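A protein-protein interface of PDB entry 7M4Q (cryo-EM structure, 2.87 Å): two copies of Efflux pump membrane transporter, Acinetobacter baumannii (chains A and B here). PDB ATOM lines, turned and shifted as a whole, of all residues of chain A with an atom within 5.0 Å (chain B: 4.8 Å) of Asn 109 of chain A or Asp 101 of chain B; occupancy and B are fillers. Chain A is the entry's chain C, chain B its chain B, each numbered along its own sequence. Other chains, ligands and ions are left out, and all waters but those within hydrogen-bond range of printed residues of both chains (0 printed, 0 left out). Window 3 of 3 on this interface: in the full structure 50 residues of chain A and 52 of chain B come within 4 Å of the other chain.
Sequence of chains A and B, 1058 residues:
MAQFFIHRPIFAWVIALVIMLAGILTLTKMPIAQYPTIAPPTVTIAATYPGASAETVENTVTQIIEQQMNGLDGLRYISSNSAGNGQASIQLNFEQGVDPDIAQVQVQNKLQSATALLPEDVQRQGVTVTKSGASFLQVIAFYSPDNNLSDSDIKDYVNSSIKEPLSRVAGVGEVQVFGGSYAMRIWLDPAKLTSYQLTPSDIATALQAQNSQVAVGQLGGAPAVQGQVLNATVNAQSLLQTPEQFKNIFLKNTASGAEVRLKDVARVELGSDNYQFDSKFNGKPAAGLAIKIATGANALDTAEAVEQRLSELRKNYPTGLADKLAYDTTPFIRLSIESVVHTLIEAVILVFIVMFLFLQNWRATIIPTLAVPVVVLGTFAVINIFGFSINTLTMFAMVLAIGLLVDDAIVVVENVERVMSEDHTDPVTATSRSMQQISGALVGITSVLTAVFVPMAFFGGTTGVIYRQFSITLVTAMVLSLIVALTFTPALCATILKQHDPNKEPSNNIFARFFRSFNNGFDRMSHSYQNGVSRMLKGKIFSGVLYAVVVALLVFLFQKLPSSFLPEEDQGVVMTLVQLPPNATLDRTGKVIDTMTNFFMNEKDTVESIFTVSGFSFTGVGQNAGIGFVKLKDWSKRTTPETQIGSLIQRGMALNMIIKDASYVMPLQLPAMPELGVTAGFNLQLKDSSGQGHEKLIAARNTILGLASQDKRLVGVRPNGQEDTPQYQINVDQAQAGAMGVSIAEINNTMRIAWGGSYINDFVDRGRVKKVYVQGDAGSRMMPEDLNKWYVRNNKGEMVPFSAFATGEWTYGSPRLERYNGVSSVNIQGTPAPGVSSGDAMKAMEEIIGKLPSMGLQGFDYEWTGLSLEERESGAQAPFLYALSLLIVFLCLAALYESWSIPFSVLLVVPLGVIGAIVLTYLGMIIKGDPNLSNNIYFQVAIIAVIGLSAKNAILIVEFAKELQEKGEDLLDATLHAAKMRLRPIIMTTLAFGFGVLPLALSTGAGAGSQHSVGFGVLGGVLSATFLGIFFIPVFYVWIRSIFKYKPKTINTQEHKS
OD2 of Asp 101 of chain B sits at hydrogen-bond distance from NE2 of Gln 106 of chain A (3.3 Å). The backbone carbonyl oxygen (O) of Asp 101 of chain B lies within hydrogen-bond range of the side-chain amide nitrogen (ND2) of Asn 109 of chain A (3.0 Å). NE2 of Gln 108 of chain B sits at hydrogen-bond distance from O of Gln 108 of chain A, 3.4 Å away. The side-chain amide nitrogen (NE2) of Gln 108 of chain B lies within hydrogen-bond range of the side-chain amide oxygen (OD1) of Asn 109 of chain A (3.0 Å).
OD1 of Asp 101 of chain B lies within salt-bridge range of NZ of Lys 131 of chain B, 3.3 Å away. NE2 of Gln 104 of chain B sits at hydrogen-bond distance from OE1 of Gln 108 of chain B, 2.9 Å away. O of Val 105 of chain A lies close to OD1 of Asn 109 of chain A (3.2 Å).
CG2 of Val 105 of chain B touches OE1 of Gln 108 of chain A (3.9 Å). Gln 104 of chain B touches Asn 109 of chain A. Val 105 of chain B touches Asn 109 of chain A (CB to OD1, 3.5 Å). OE1 of Gln 108 of chain B touches CG of Gln 112 of chain A, 3.4 Å away.
Of the printed residues of chain B, Gln 106 of chain A touches Asp 101. Of the printed residues of chain B, Gln 108 of chain A touches Val 105 and Gln 108. Asn 109 of chain A touches four residues of chain B. Printed residues of chain B within 4 Å of Gln 112 of chain A: Gln 108 (3.4 Å). Asp 101 of chain B touches just these residues of chain A: Gln 106 (3.3 Å) and Asn 109 (3.0 Å). Ile 102 of chain B touches none of the printed residues of chain A. Ala 103 of chain B touches none of the printed residues of chain A. Printed residues of chain A within 4 Å of Val 105 of chain B: Gln 108 (3.9 Å) and Asn 109 (3.5 Å).
Of the 9 printed residues of chain B, 4 touch a printed residue of chain A. Hydrophobic or aromatic side chains of chain B that line the printed part of chain A: Val 105. Of the 9 printed residues of chain A, 4 touch a printed residue of chain B.
Gln 108 of chain A touches Val 105 of chain B, but with the chains exchanged Val 105 of chain A does not touch Gln 108 of chain B (5.2 Å). Gln 108 of chain A touches its own counterpart, Gln 108 of chain B. Of the 8 pairs that touch across the chains among the printed residues, 1 has its exchanged pair printed and touching as well.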
ATOM      1  N   VAL A 105     -13.135 -21.208  12.078  1.00  0.00           N
ATOM      2  CA  VAL A 105     -13.283 -20.384  10.878  1.00  0.00           C
ATOM      3  C   VAL A 105     -12.582 -21.033   9.691  1.00  0.00           C
ATOM      4  O   VAL A 105     -13.055 -20.933   8.559  1.00  0.00           O
ATOM      5  CB  VAL A 105     -12.806 -18.928  11.085  1.00  0.00           C
ATOM      6  CG1 VAL A 105     -13.097 -18.444  12.486  1.00  0.00           C
ATOM      7  CG2 VAL A 105     -11.346 -18.748  10.723  1.00  0.00           C
ATOM      8  N   GLN A 106     -11.458 -21.714   9.914  1.00  0.00           N
ATOM      9  CA  GLN A 106     -10.783 -22.357   8.790  1.00  0.00           C
ATOM     10  C   GLN A 106     -11.559 -23.567   8.278  1.00  0.00           C
ATOM     11  O   GLN A 106     -11.587 -23.832   7.068  1.00  0.00           O
ATOM     12  CB  GLN A 106      -9.373 -22.743   9.191  1.00  0.00           C
ATOM     13  CG  GLN A 106      -8.465 -21.560   9.302  1.00  0.00           C
ATOM     14  CD  GLN A 106      -7.141 -21.913   9.900  1.00  0.00           C
ATOM     15  OE1 GLN A 106      -6.727 -23.066   9.886  1.00  0.00           O
ATOM     16  NE2 GLN A 106      -6.466 -20.919  10.447  1.00  0.00           N
ATOM     17  N   VAL A 107     -12.210 -24.304   9.177  1.00  0.00           N
ATOM     18  CA  VAL A 107     -13.113 -25.356   8.733  1.00  0.00           C
ATOM     19  C   VAL A 107     -14.219 -24.762   7.875  1.00  0.00           C
ATOM     20  O   VAL A 107     -14.579 -25.320   6.841  1.00  0.00           O
ATOM     21  CB  VAL A 107     -13.679 -26.133   9.939  1.00  0.00           C
ATOM     22  CG1 VAL A 107     -14.683 -27.173   9.492  1.00  0.00           C
ATOM     23  CG2 VAL A 107     -12.564 -26.790  10.721  1.00  0.00           C
ATOM     24  N   GLN A 108     -14.785 -23.630   8.301  1.00  0.00           N
ATOM     25  CA  GLN A 108     -15.840 -22.994   7.510  1.00  0.00           C
ATOM     26  C   GLN A 108     -15.323 -22.521   6.158  1.00  0.00           C
ATOM     27  O   GLN A 108     -16.037 -22.601   5.154  1.00  0.00           O
ATOM     28  CB  GLN A 108     -16.445 -21.823   8.272  1.00  0.00           C
ATOM     29  CG  GLN A 108     -17.424 -22.225   9.321  1.00  0.00           C
ATOM     30  CD  GLN A 108     -17.786 -21.088  10.224  1.00  0.00           C
ATOM     31  OE1 GLN A 108     -17.575 -19.933   9.894  1.00  0.00           O
ATOM     32  NE2 GLN A 108     -18.332 -21.409  11.380  1.00  0.00           N
ATOM     33  N   ASN A 109     -14.093 -22.011   6.116  1.00  0.00           N
ATOM     34  CA  ASN A 109     -13.516 -21.539   4.862  1.00  0.00           C
ATOM     35  C   ASN A 109     -13.314 -22.675   3.870  1.00  0.00           C
ATOM     36  O   ASN A 109     -13.527 -22.500   2.668  1.00  0.00           O
ATOM     37  CB  ASN A 109     -12.200 -20.812   5.131  1.00  0.00           C
ATOM     38  CG  ASN A 109     -12.408 -19.431   5.721  1.00  0.00           C
ATOM     39  OD1 ASN A 109     -13.518 -19.050   6.051  1.00  0.00           O
ATOM     40  ND2 ASN A 109     -11.339 -18.686   5.862  1.00  0.00           N
ATOM     41  N   LYS A 110     -12.901 -23.849   4.345  1.00  0.00           N
ATOM     42  CA  LYS A 110     -12.802 -24.991   3.434  1.00  0.00           C
ATOM     43  C   LYS A 110     -14.169 -25.584   3.098  1.00  0.00           C
ATOM     44  O   LYS A 110     -14.409 -26.000   1.955  1.00  0.00           O
ATOM     45  CB  LYS A 110     -11.878 -26.046   4.030  1.00  0.00           C
ATOM     46  CG  LYS A 110     -10.494 -25.960   3.450  1.00  0.00           C
ATOM     47  CD  LYS A 110      -9.455 -26.533   4.361  1.00  0.00           C
ATOM     48  CE  LYS A 110      -8.073 -26.116   3.908  1.00  0.00           C
ATOM     49  NZ  LYS A 110      -7.041 -26.312   4.957  1.00  0.00           N
ATOM     50  N   LEU A 111     -15.087 -25.587   4.056  1.00  0.00           N
ATOM     51  CA  LEU A 111     -16.405 -26.160   3.833  1.00  0.00           C
ATOM     52  C   LEU A 111     -17.222 -25.337   2.851  1.00  0.00           C
ATOM     53  O   LEU A 111     -18.067 -25.888   2.140  1.00  0.00           O
ATOM     54  CB  LEU A 111     -17.128 -26.274   5.169  1.00  0.00           C
ATOM     55  CG  LEU A 111     -18.440 -27.039   5.241  1.00  0.00           C
ATOM     56  CD1 LEU A 111     -18.252 -28.511   4.968  1.00  0.00           C
ATOM     57  CD2 LEU A 111     -19.023 -26.825   6.611  1.00  0.00           C
ATOM     58  N   GLN A 112     -16.994 -24.025   2.807  1.00  0.00           N
ATOM     59  CA  GLN A 112     -17.700 -23.174   1.857  1.00  0.00           C
ATOM     60  C   GLN A 112     -17.579 -23.720   0.445  1.00  0.00           C
ATOM     61  O   GLN A 112     -18.579 -23.897  -0.254  1.00  0.00           O
ATOM     62  CB  GLN A 112     -17.137 -21.750   1.949  1.00  0.00           C
ATOM     63  CG  GLN A 112     -17.402 -20.856   0.758  1.00  0.00           C
ATOM     64  CD  GLN A 112     -18.856 -20.538   0.614  1.00  0.00           C
ATOM     65  OE1 GLN A 112     -19.576 -20.474   1.607  1.00  0.00           O
ATOM     66  NE2 GLN A 112     -19.310 -20.356  -0.617  1.00  0.00           N
ATOM     67  N   SER A 113     -16.353 -24.002   0.012  1.00  0.00           N
ATOM     68  CA  SER A 113     -16.147 -24.537  -1.326  1.00  0.00           C
ATOM     69  C   SER A 113     -16.538 -26.006  -1.399  1.00  0.00           C
ATOM     70  O   SER A 113     -17.068 -26.460  -2.417  1.00  0.00           O
ATOM     71  CB  SER A 113     -14.693 -24.342  -1.737  1.00  0.00           C
ATOM     72  OG  SER A 113     -14.397 -25.057  -2.921  1.00  0.00           O
ATOM     73  N   ASP B  99      -5.469 -10.654   8.076  1.00  0.00           N
ATOM     74  CA  ASP B  99      -5.523 -12.102   8.149  1.00  0.00           C
ATOM     75  C   ASP B  99      -6.334 -12.646   6.980  1.00  0.00           C
ATOM     76  O   ASP B  99      -7.523 -12.323   6.865  1.00  0.00           O
ATOM     77  CB  ASP B  99      -6.160 -12.525   9.469  1.00  0.00           C
ATOM     78  CG  ASP B  99      -6.002 -14.009   9.766  1.00  0.00           C
ATOM     79  OD1 ASP B  99      -5.189 -14.685   9.107  1.00  0.00           O
ATOM     80  OD2 ASP B  99      -6.688 -14.494  10.683  1.00  0.00           O
ATOM     81  N   PRO B 100      -5.751 -13.460   6.100  1.00  0.00           N
ATOM     82  CA  PRO B 100      -6.524 -13.973   4.959  1.00  0.00           C
ATOM     83  C   PRO B 100      -7.737 -14.804   5.343  1.00  0.00           C
ATOM     84  O   PRO B 100      -8.761 -14.754   4.652  1.00  0.00           O
ATOM     85  CB  PRO B 100      -5.477 -14.791   4.205  1.00  0.00           C
ATOM     86  CG  PRO B 100      -4.211 -14.131   4.530  1.00  0.00           C
ATOM     87  CD  PRO B 100      -4.323 -13.765   5.955  1.00  0.00           C
ATOM     88  N   ASP B 101      -7.649 -15.566   6.432  1.00  0.00           N
ATOM     89  CA  ASP B 101      -8.764 -16.411   6.841  1.00  0.00           C
ATOM     90  C   ASP B 101      -9.964 -15.576   7.277  1.00  0.00           C
ATOM     91  O   ASP B 101     -11.110 -15.893   6.933  1.00  0.00           O
ATOM     92  CB  ASP B 101      -8.312 -17.349   7.958  1.00  0.00           C
ATOM     93  CG  ASP B 101      -7.621 -18.604   7.436  1.00  0.00           C
ATOM     94  OD1 ASP B 101      -8.214 -19.342   6.625  1.00  0.00           O
ATOM     95  OD2 ASP B 101      -6.475 -18.866   7.844  1.00  0.00           O
ATOM     96  N   ILE B 102      -9.720 -14.501   8.024  1.00  0.00           N
ATOM     97  CA  ILE B 102     -10.801 -13.619   8.443  1.00  0.00           C
ATOM     98  C   ILE B 102     -11.405 -12.907   7.241  1.00  0.00           C
ATOM     99  O   ILE B 102     -12.624 -12.735   7.150  1.00  0.00           O
ATOM    100  CB  ILE B 102     -10.292 -12.615   9.492  1.00  0.00           C
ATOM    101  CG1 ILE B 102      -9.645 -13.334  10.675  1.00  0.00           C
ATOM    102  CG2 ILE B 102     -11.419 -11.721   9.967  1.00  0.00           C
ATOM    103  CD1 ILE B 102     -10.570 -14.205  11.495  1.00  0.00           C
ATOM    104  N   ALA B 103     -10.569 -12.452   6.315  1.00  0.00           N
ATOM    105  CA  ALA B 103     -11.102 -11.786   5.137  1.00  0.00           C
ATOM    106  C   ALA B 103     -12.014 -12.720   4.356  1.00  0.00           C
ATOM    107  O   ALA B 103     -13.097 -12.321   3.916  1.00  0.00           O
ATOM    108  CB  ALA B 103      -9.957 -11.281   4.271  1.00  0.00           C
ATOM    109  N   GLN B 104     -11.604 -13.980   4.199  1.00  0.00           N
ATOM    110  CA  GLN B 104     -12.433 -14.931   3.472  1.00  0.00           C
ATOM    111  C   GLN B 104     -13.739 -15.211   4.201  1.00  0.00           C
ATOM    112  O   GLN B 104     -14.806 -15.246   3.579  1.00  0.00           O
ATOM    113  CB  GLN B 104     -11.670 -16.230   3.241  1.00  0.00           C
ATOM    114  CG  GLN B 104     -12.095 -16.932   1.986  1.00  0.00           C
ATOM    115  CD  GLN B 104     -11.970 -18.418   2.064  1.00  0.00           C
ATOM    116  OE1 GLN B 104     -10.904 -18.946   2.343  1.00  0.00           O
ATOM    117  NE2 GLN B 104     -13.057 -19.109   1.813  1.00  0.00           N
ATOM    118  N   VAL B 105     -13.677 -15.426   5.516  1.00  0.00           N
ATOM    119  CA  VAL B 105     -14.892 -15.737   6.262  1.00  0.00           C
ATOM    120  C   VAL B 105     -15.855 -14.555   6.227  1.00  0.00           C
ATOM    121  O   VAL B 105     -17.067 -14.729   6.076  1.00  0.00           O
ATOM    122  CB  VAL B 105     -14.546 -16.170   7.704  1.00  0.00           C
ATOM    123  CG1 VAL B 105     -14.239 -14.992   8.581  1.00  0.00           C
ATOM    124  CG2 VAL B 105     -15.650 -17.004   8.299  1.00  0.00           C
ATOM    125  N   GLN B 108     -17.519 -14.423   2.694  1.00  0.00           N
ATOM    126  CA  GLN B 108     -18.530 -15.452   2.475  1.00  0.00           C
ATOM    127  C   GLN B 108     -19.681 -15.358   3.469  1.00  0.00           C
ATOM    128  O   GLN B 108     -20.739 -15.936   3.215  1.00  0.00           O
ATOM    129  CB  GLN B 108     -17.900 -16.850   2.504  1.00  0.00           C
ATOM    130  CG  GLN B 108     -17.339 -17.262   3.836  1.00  0.00           C
ATOM    131  CD  GLN B 108     -16.396 -18.439   3.745  1.00  0.00           C
ATOM    132  OE1 GLN B 108     -15.770 -18.674   2.719  1.00  0.00           O
ATOM    133  NE2 GLN B 108     -16.284 -19.180   4.829  1.00  0.00           N
ATOM    134  N   LYS B 131      -9.395 -17.815  -1.726  1.00  0.00           N
ATOM    135  CA  LYS B 131      -8.399 -16.768  -1.547  1.00  0.00           C
ATOM    136  C   LYS B 131      -7.092 -17.139  -2.233  1.00  0.00           C
ATOM    137  O   LYS B 131      -6.877 -18.278  -2.644  1.00  0.00           O
ATOM    138  CB  LYS B 131      -8.161 -16.465  -0.071  1.00  0.00           C
ATOM    139  CG  LYS B 131      -7.924 -17.653   0.776  1.00  0.00           C
ATOM    140  CD  LYS B 131      -7.341 -17.216   2.081  1.00  0.00           C
ATOM    141  CE  LYS B 131      -7.419 -18.289   3.101  1.00  0.00           C
ATOM    142  NZ  LYS B 131      -6.535 -17.935   4.212  1.00  0.00           N
